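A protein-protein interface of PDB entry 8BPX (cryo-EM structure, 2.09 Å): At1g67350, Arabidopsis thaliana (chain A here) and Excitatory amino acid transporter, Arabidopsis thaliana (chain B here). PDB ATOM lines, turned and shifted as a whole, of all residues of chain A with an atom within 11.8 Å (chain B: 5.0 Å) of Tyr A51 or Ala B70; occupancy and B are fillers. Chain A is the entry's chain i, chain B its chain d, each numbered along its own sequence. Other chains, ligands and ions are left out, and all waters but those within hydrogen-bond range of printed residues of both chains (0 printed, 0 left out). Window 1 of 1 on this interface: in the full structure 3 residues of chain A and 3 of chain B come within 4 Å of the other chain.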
ATOM      1  N   ALA A  45     -11.752  16.879 -20.257  1.00  0.00           N
ATOM      2  CA  ALA A  45     -12.583  16.630 -21.427  1.00  0.00           C
ATOM      3  C   ALA A  45     -13.878  17.433 -21.421  1.00  0.00           C
ATOM      4  O   ALA A  45     -14.674  17.298 -22.356  1.00  0.00           O
ATOM      5  CB  ALA A  45     -12.908  15.136 -21.535  1.00  0.00           C
ATOM      6  N   LEU A  46     -14.106  18.255 -20.402  1.00  0.00           N
ATOM      7  CA  LEU A  46     -15.327  19.050 -20.341  1.00  0.00           C
ATOM      8  C   LEU A  46     -15.333  20.074 -21.470  1.00  0.00           C
ATOM      9  O   LEU A  46     -14.334  20.778 -21.667  1.00  0.00           O
ATOM     10  CB  LEU A  46     -15.443  19.756 -18.990  1.00  0.00           C
ATOM     11  CG  LEU A  46     -16.499  19.232 -18.013  1.00  0.00           C
ATOM     12  CD1 LEU A  46     -16.300  19.841 -16.636  1.00  0.00           C
ATOM     13  CD2 LEU A  46     -17.901  19.515 -18.521  1.00  0.00           C
ATOM     14  N   PRO A  47     -16.418  20.183 -22.234  1.00  0.00           N
ATOM     15  CA  PRO A  47     -16.440  21.140 -23.346  1.00  0.00           C
ATOM     16  C   PRO A  47     -16.346  22.575 -22.849  1.00  0.00           C
ATOM     17  O   PRO A  47     -16.995  22.959 -21.873  1.00  0.00           O
ATOM     18  CB  PRO A  47     -17.787  20.861 -24.022  1.00  0.00           C
ATOM     19  CG  PRO A  47     -18.629  20.286 -22.935  1.00  0.00           C
ATOM     20  CD  PRO A  47     -17.687  19.446 -22.123  1.00  0.00           C
ATOM     21  N   ILE A  48     -15.600  23.433 -23.519  1.00  0.00           N
ATOM     22  CA  ILE A  48     -15.556  24.844 -23.088  1.00  0.00           C
ATOM     23  C   ILE A  48     -16.860  25.506 -23.555  1.00  0.00           C
ATOM     24  O   ILE A  48     -17.326  26.452 -22.880  1.00  0.00           O
ATOM     25  CB  ILE A  48     -14.281  25.482 -23.686  1.00  0.00           C
ATOM     26  CG1 ILE A  48     -14.071  26.943 -23.302  1.00  0.00           C
ATOM     27  CG2 ILE A  48     -14.269  25.311 -25.199  1.00  0.00           C
ATOM     28  CD1 ILE A  48     -12.992  27.600 -24.120  1.00  0.00           C
ATOM     29  N   ARG A  49     -17.396  25.029 -24.686  1.00  0.00           N
ATOM     30  CA  ARG A  49     -18.684  25.536 -25.139  1.00  0.00           C
ATOM     31  C   ARG A  49     -19.745  24.503 -24.792  1.00  0.00           C
ATOM     32  O   ARG A  49     -19.865  23.480 -25.485  1.00  0.00           O
ATOM     33  CB  ARG A  49     -18.646  25.800 -26.648  1.00  0.00           C
ATOM     34  CG  ARG A  49     -19.813  26.587 -27.214  1.00  0.00           C
ATOM     35  CD  ARG A  49     -20.934  25.658 -27.660  1.00  0.00           C
ATOM     36  NE  ARG A  49     -20.505  24.754 -28.721  1.00  0.00           N
ATOM     37  CZ  ARG A  49     -21.262  23.798 -29.241  1.00  0.00           C
ATOM     38  NH1 ARG A  49     -22.502  23.595 -28.825  1.00  0.00           N
ATOM     39  NH2 ARG A  49     -20.764  23.028 -30.205  1.00  0.00           N
ATOM     40  N   PRO A  50     -20.513  24.730 -23.693  1.00  0.00           N
ATOM     41  CA  PRO A  50     -21.484  23.728 -23.290  1.00  0.00           C
ATOM     42  C   PRO A  50     -22.567  23.494 -24.355  1.00  0.00           C
ATOM     43  O   PRO A  50     -22.680  24.287 -25.255  1.00  0.00           O
ATOM     44  CB  PRO A  50     -21.981  24.322 -21.952  1.00  0.00           C
ATOM     45  CG  PRO A  50     -21.841  25.789 -22.080  1.00  0.00           C
ATOM     46  CD  PRO A  50     -20.524  25.901 -22.789  1.00  0.00           C
ATOM     47  N   TYR A  51     -23.307  22.417 -24.249  1.00  0.00           N
ATOM     48  CA  TYR A  51     -24.415  22.109 -25.142  1.00  0.00           C
ATOM     49  C   TYR A  51     -25.538  23.120 -24.962  1.00  0.00           C
ATOM     50  O   TYR A  51     -26.142  23.205 -23.888  1.00  0.00           O
ATOM     51  CB  TYR A  51     -24.917  20.695 -24.858  1.00  0.00           C
ATOM     52  CG  TYR A  51     -25.746  20.070 -25.956  1.00  0.00           C
ATOM     53  CD1 TYR A  51     -25.363  20.161 -27.285  1.00  0.00           C
ATOM     54  CD2 TYR A  51     -26.911  19.378 -25.657  1.00  0.00           C
ATOM     55  CE1 TYR A  51     -26.118  19.583 -28.287  1.00  0.00           C
ATOM     56  CE2 TYR A  51     -27.671  18.797 -26.648  1.00  0.00           C
ATOM     57  CZ  TYR A  51     -27.271  18.900 -27.961  1.00  0.00           C
ATOM     58  OH  TYR A  51     -28.032  18.320 -28.945  1.00  0.00           O
ATOM     59  N   GLY A  52     -25.821  23.882 -26.016  1.00  0.00           N
ATOM     60  CA  GLY A  52     -26.912  24.835 -25.991  1.00  0.00           C
ATOM     61  C   GLY A  52     -26.764  25.910 -24.934  1.00  0.00           C
ATOM     62  O   GLY A  52     -27.697  26.154 -24.168  1.00  0.00           O
ATOM     63  N   PHE A  53     -25.593  26.549 -24.868  1.00  0.00           N
ATOM     64  CA  PHE A  53     -25.379  27.567 -23.845  1.00  0.00           C
ATOM     65  C   PHE A  53     -26.350  28.730 -24.013  1.00  0.00           C
ATOM     66  O   PHE A  53     -26.837  29.288 -23.025  1.00  0.00           O
ATOM     67  CB  PHE A  53     -23.934  28.061 -23.877  1.00  0.00           C
ATOM     68  CG  PHE A  53     -23.537  28.707 -25.173  1.00  0.00           C
ATOM     69  CD1 PHE A  53     -23.087  27.943 -26.236  1.00  0.00           C
ATOM     70  CD2 PHE A  53     -23.605  30.080 -25.327  1.00  0.00           C
ATOM     71  CE1 PHE A  53     -22.720  28.540 -27.426  1.00  0.00           C
ATOM     72  CE2 PHE A  53     -23.241  30.677 -26.516  1.00  0.00           C
ATOM     73  CZ  PHE A  53     -22.798  29.910 -27.563  1.00  0.00           C
ATOM     74  N   TRP A  54     -26.668  29.089 -25.260  1.00  0.00           N
ATOM     75  CA  TRP A  54     -27.600  30.178 -25.528  1.00  0.00           C
ATOM     76  C   TRP A  54     -29.007  29.887 -25.021  1.00  0.00           C
ATOM     77  O   TRP A  54     -29.826  30.810 -24.959  1.00  0.00           O
ATOM     78  CB  TRP A  54     -27.628  30.476 -27.028  1.00  0.00           C
ATOM     79  CG  TRP A  54     -28.080  29.306 -27.830  1.00  0.00           C
ATOM     80  CD1 TRP A  54     -29.356  28.986 -28.153  1.00  0.00           C
ATOM     81  CD2 TRP A  54     -27.253  28.276 -28.384  1.00  0.00           C
ATOM     82  NE1 TRP A  54     -29.385  27.824 -28.885  1.00  0.00           N
ATOM     83  CE2 TRP A  54     -28.104  27.366 -29.040  1.00  0.00           C
ATOM     84  CE3 TRP A  54     -25.878  28.036 -28.392  1.00  0.00           C
ATOM     85  CZ2 TRP A  54     -27.624  26.241 -29.703  1.00  0.00           C
ATOM     86  CZ3 TRP A  54     -25.403  26.917 -29.047  1.00  0.00           C
ATOM     87  CH2 TRP A  54     -26.273  26.033 -29.694  1.00  0.00           C
ATOM     88  N   THR A  55     -29.309  28.634 -24.672  1.00  0.00           N
ATOM     89  CA  THR A  55     -30.558  28.295 -24.000  1.00  0.00           C
ATOM     90  C   THR A  55     -30.592  28.766 -22.551  1.00  0.00           C
ATOM     91  O   THR A  55     -31.682  29.008 -22.017  1.00  0.00           O
ATOM     92  CB  THR A  55     -30.776  26.778 -24.068  1.00  0.00           C
ATOM     93  OG1 THR A  55     -30.740  26.352 -25.435  1.00  0.00           O
ATOM     94  CG2 THR A  55     -32.104  26.369 -23.449  1.00  0.00           C
ATOM     95  N   PHE A  56     -29.425  28.902 -21.894  1.00  0.00           N
ATOM     96  CA  PHE A  56     -29.319  29.260 -20.467  1.00  0.00           C
ATOM     97  C   PHE A  56     -29.965  30.643 -20.217  1.00  0.00           C
ATOM     98  O   PHE A  56     -29.711  31.567 -21.011  1.00  0.00           O
ATOM     99  CB  PHE A  56     -27.874  29.125 -20.011  1.00  0.00           C
ATOM    100  CG  PHE A  56     -27.152  27.826 -20.259  1.00  0.00           C
ATOM    101  CD1 PHE A  56     -27.832  26.640 -20.465  1.00  0.00           C
ATOM    102  CD2 PHE A  56     -25.767  27.800 -20.287  1.00  0.00           C
ATOM    103  CE1 PHE A  56     -27.147  25.462 -20.705  1.00  0.00           C
ATOM    104  CE2 PHE A  56     -25.081  26.622 -20.541  1.00  0.00           C
ATOM    105  CZ  PHE A  56     -25.775  25.456 -20.743  1.00  0.00           C
ATOM    106  N   GLU A  57     -30.762  30.777 -19.165  1.00  0.00           N
ATOM    107  CA  GLU A  57     -31.616  31.937 -18.930  1.00  0.00           C
ATOM    108  C   GLU A  57     -30.841  33.247 -18.980  1.00  0.00           C
ATOM    109  O   GLU A  57     -31.381  34.266 -19.424  1.00  0.00           O
ATOM    110  CB  GLU A  57     -32.328  31.798 -17.584  1.00  0.00           C
ATOM    111  CG  GLU A  57     -33.537  30.878 -17.616  1.00  0.00           C
ATOM    112  CD  GLU A  57     -33.154  29.410 -17.686  1.00  0.00           C
ATOM    113  OE1 GLU A  57     -31.989  29.082 -17.376  1.00  0.00           O
ATOM    114  OE2 GLU A  57     -34.018  28.585 -18.050  1.00  0.00           O
ATOM    115  N   HIS A  59     -28.788  34.106 -20.993  1.00  0.00           N
ATOM    116  CA  HIS A  59     -28.589  34.522 -22.390  1.00  0.00           C
ATOM    117  C   HIS A  59     -29.910  34.903 -23.094  1.00  0.00           C
ATOM    118  O   HIS A  59     -29.876  35.305 -24.232  1.00  0.00           O
ATOM    119  CB  HIS A  59     -27.840  33.405 -23.048  1.00  0.00           C
ATOM    120  CG  HIS A  59     -26.599  32.925 -22.361  1.00  0.00           C
ATOM    121  ND1 HIS A  59     -25.819  31.931 -22.894  1.00  0.00           N
ATOM    122  CD2 HIS A  59     -26.011  33.269 -21.196  1.00  0.00           C
ATOM    123  CE1 HIS A  59     -24.808  31.681 -22.093  1.00  0.00           C
ATOM    124  NE2 HIS A  59     -24.905  32.485 -21.041  1.00  0.00           N
ATOM    125  N   ASN A  60     -31.026  34.712 -22.433  1.00  0.00           N
ATOM    126  CA  ASN A  60     -32.328  35.019 -23.012  1.00  0.00           C
ATOM    127  C   ASN A  60     -32.893  36.317 -22.440  1.00  0.00           C
ATOM    128  O   ASN A  60     -34.100  36.451 -22.235  1.00  0.00           O
ATOM    129  CB  ASN A  60     -33.306  33.868 -22.792  1.00  0.00           C
ATOM    130  CG  ASN A  60     -32.957  32.641 -23.615  1.00  0.00           C
ATOM    131  OD1 ASN A  60     -32.291  32.736 -24.647  1.00  0.00           O
ATOM    132  ND2 ASN A  60     -33.411  31.477 -23.159  1.00  0.00           N
ATOM    133  N   LYS B  66     -23.176  22.308 -12.299  1.00  0.00           N
ATOM    134  CA  LYS B  66     -24.043  22.809 -13.362  1.00  0.00           C
ATOM    135  C   LYS B  66     -23.436  22.557 -14.737  1.00  0.00           C
ATOM    136  O   LYS B  66     -24.150  22.190 -15.680  1.00  0.00           O
ATOM    137  CB  LYS B  66     -24.327  24.296 -13.167  1.00  0.00           C
ATOM    138  CG  LYS B  66     -25.164  24.607 -11.940  1.00  0.00           C
ATOM    139  CD  LYS B  66     -25.410  26.101 -11.760  1.00  0.00           C
ATOM    140  CE  LYS B  66     -26.267  26.410 -10.545  1.00  0.00           C
ATOM    141  NZ  LYS B  66     -26.468  27.875 -10.384  1.00  0.00           N
ATOM    142  N   ALA B  67     -22.123  22.758 -14.875  1.00  0.00           N
ATOM    143  CA  ALA B  67     -21.471  22.457 -16.147  1.00  0.00           C
ATOM    144  C   ALA B  67     -21.648  20.989 -16.520  1.00  0.00           C
ATOM    145  O   ALA B  67     -21.955  20.665 -17.675  1.00  0.00           O
ATOM    146  CB  ALA B  67     -19.989  22.820 -16.081  1.00  0.00           C
ATOM    147  N   ARG B  68     -21.465  20.090 -15.550  1.00  0.00           N
ATOM    148  CA  ARG B  68     -21.625  18.662 -15.807  1.00  0.00           C
ATOM    149  C   ARG B  68     -23.053  18.325 -16.209  1.00  0.00           C
ATOM    150  O   ARG B  68     -23.271  17.507 -17.108  1.00  0.00           O
ATOM    151  CB  ARG B  68     -21.226  17.855 -14.572  1.00  0.00           C
ATOM    152  CG  ARG B  68     -19.870  17.182 -14.674  1.00  0.00           C
ATOM    153  CD  ARG B  68     -19.399  16.720 -13.307  1.00  0.00           C
ATOM    154  NE  ARG B  68     -19.160  17.844 -12.408  1.00  0.00           N
ATOM    155  CZ  ARG B  68     -19.322  17.797 -11.092  1.00  0.00           C
ATOM    156  NH1 ARG B  68     -19.728  16.695 -10.484  1.00  0.00           N
ATOM    157  NH2 ARG B  68     -19.071  18.883 -10.370  1.00  0.00           N
ATOM    158  N   ALA B  69     -24.040  18.921 -15.536  1.00  0.00           N
ATOM    159  CA  ALA B  69     -25.433  18.672 -15.901  1.00  0.00           C
ATOM    160  C   ALA B  69     -25.722  19.142 -17.320  1.00  0.00           C
ATOM    161  O   ALA B  69     -26.377  18.435 -18.101  1.00  0.00           O
ATOM    162  CB  ALA B  69     -26.370  19.363 -14.913  1.00  0.00           C
ATOM    163  N   ALA B  70     -25.240  20.336 -17.673  1.00  0.00           N
ATOM    164  CA  ALA B  70     -25.460  20.847 -19.020  1.00  0.00           C
ATOM    165  C   ALA B  70     -24.819  19.940 -20.060  1.00  0.00           C
ATOM    166  O   ALA B  70     -25.399  19.694 -21.122  1.00  0.00           O
ATOM    167  CB  ALA B  70     -24.916  22.271 -19.138  1.00  0.00           C
ATOM    168  N   ASN B  71     -23.616  19.436 -19.770  1.00  0.00           N
ATOM    169  CA  ASN B  71     -22.964  18.513 -20.693  1.00  0.00           C
ATOM    170  C   ASN B  71     -23.734  17.203 -20.812  1.00  0.00           C
ATOM    171  O   ASN B  71     -23.905  16.675 -21.916  1.00  0.00           O
ATOM    172  CB  ASN B  71     -21.527  18.250 -20.244  1.00  0.00           C
ATOM    173  CG  ASN B  71     -20.728  17.482 -21.275  1.00  0.00           C
ATOM    174  OD1 ASN B  71     -20.688  17.853 -22.446  1.00  0.00           O
ATOM    175  ND2 ASN B  71     -20.089  16.402 -20.843  1.00  0.00           N
ATOM    176  N   GLU B  72     -24.204  16.663 -19.685  1.00  0.00           N
ATOM    177  CA  GLU B  72     -24.933  15.400 -19.693  1.00  0.00           C
ATOM    178  C   GLU B  72     -26.277  15.516 -20.392  1.00  0.00           C
ATOM    179  O   GLU B  72     -26.820  14.500 -20.840  1.00  0.00           O
ATOM    180  CB  GLU B  72     -25.135  14.899 -18.264  1.00  0.00           C
ATOM    181  CG  GLU B  72     -23.853  14.493 -17.559  1.00  0.00           C
ATOM    182  CD  GLU B  72     -24.090  14.072 -16.123  1.00  0.00           C
ATOM    183  OE1 GLU B  72     -25.217  14.276 -15.623  1.00  0.00           O
ATOM    184  OE2 GLU B  72     -23.154  13.539 -15.496  1.00  0.00           O
ATOM    185  N   ARG B  73     -26.829  16.728 -20.487  1.00  0.00           N
ATOM    186  CA  ARG B  73     -28.063  16.915 -21.242  1.00  0.00           C
ATOM    187  C   ARG B  73     -27.907  16.551 -22.715  1.00  0.00           C
ATOM    188  O   ARG B  73     -28.916  16.335 -23.395  1.00  0.00           O
ATOM    189  CB  ARG B  73     -28.548  18.359 -21.113  1.00  0.00           C
ATOM    190  CG  ARG B  73     -29.187  18.679 -19.774  1.00  0.00           C
ATOM    191  CD  ARG B  73     -30.379  17.776 -19.504  1.00  0.00           C
ATOM    192  NE  ARG B  73     -31.536  18.141 -20.314  1.00  0.00           N
ATOM    193  CZ  ARG B  73     -32.384  19.113 -20.011  1.00  0.00           C
ATOM    194  NH1 ARG B  73     -32.238  19.842 -18.917  1.00  0.00           N
ATOM    195  NH2 ARG B  73     -33.406  19.360 -20.825  1.00  0.00           N
ATOM    196  N   ARG B  74     -26.672  16.486 -23.223  1.00  0.00           N
ATOM    197  CA  ARG B  74     -26.463  16.157 -24.631  1.00  0.00           C
ATOM    198  C   ARG B  74     -26.920  14.740 -24.955  1.00  0.00           C
ATOM    199  O   ARG B  74     -27.517  14.500 -26.011  1.00  0.00           O
ATOM    200  CB  ARG B  74     -24.991  16.336 -25.004  1.00  0.00           C
ATOM    201  CG  ARG B  74     -24.770  16.646 -26.475  1.00  0.00           C
ATOM    202  CD  ARG B  74     -23.297  16.632 -26.852  1.00  0.00           C
ATOM    203  NE  ARG B  74     -22.564  17.745 -26.263  1.00  0.00           N
ATOM    204  CZ  ARG B  74     -21.621  17.618 -25.340  1.00  0.00           C
ATOM    205  NH1 ARG B  74     -21.260  16.433 -24.879  1.00  0.00           N
ATOM    206  NH2 ARG B  74     -21.020  18.710 -24.873  1.00  0.00           N
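Tyr A51 touches just these residues of chain B: Ala B70 and Arg B74.
Of chain A, only Tyr A51 (3.9 Å) and Phe A56 (3.7 Å) come within 4 Å of Ala B70.
Asn B71 touches just one residue of chain A: Pro A47 (3.2 Å).
Arg B74 touches just these residues of chain A: Pro A47 (3.5 Å) and Tyr A51 (3.4 Å).
Of the printed residues of chain B, Phe A56 touches Ala B70 (3.7 Å).
Printed residues of chain B within 4 Å of Pro A47: Asn B71 and Arg B74.
Pro A50 touches none of the printed residues of chain B.
Arg A49 touches none of the printed residues of chain B.
The side-chain amide oxygen of Asn B71 is in hydrogen-bond range of the guanidinium group of Arg B74 (2.6 Å).
Among the printed residues, pairs that only touch across the chains: Pro A47 with Asn B71, Tyr A51 with Arg B74, Pro A47 with Arg B74, Phe A56 with Ala B70 and Tyr A51 with Ala B70.
Hydrophobic or aromatic side chains of chain A that line the printed part of chain B: Pro A47, Tyr A51 and Phe A56.
Among the printed residues, no Asp or Glu carboxylate lies within 4 Å of a Lys or Arg side-chain nitrogen of the other chain.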
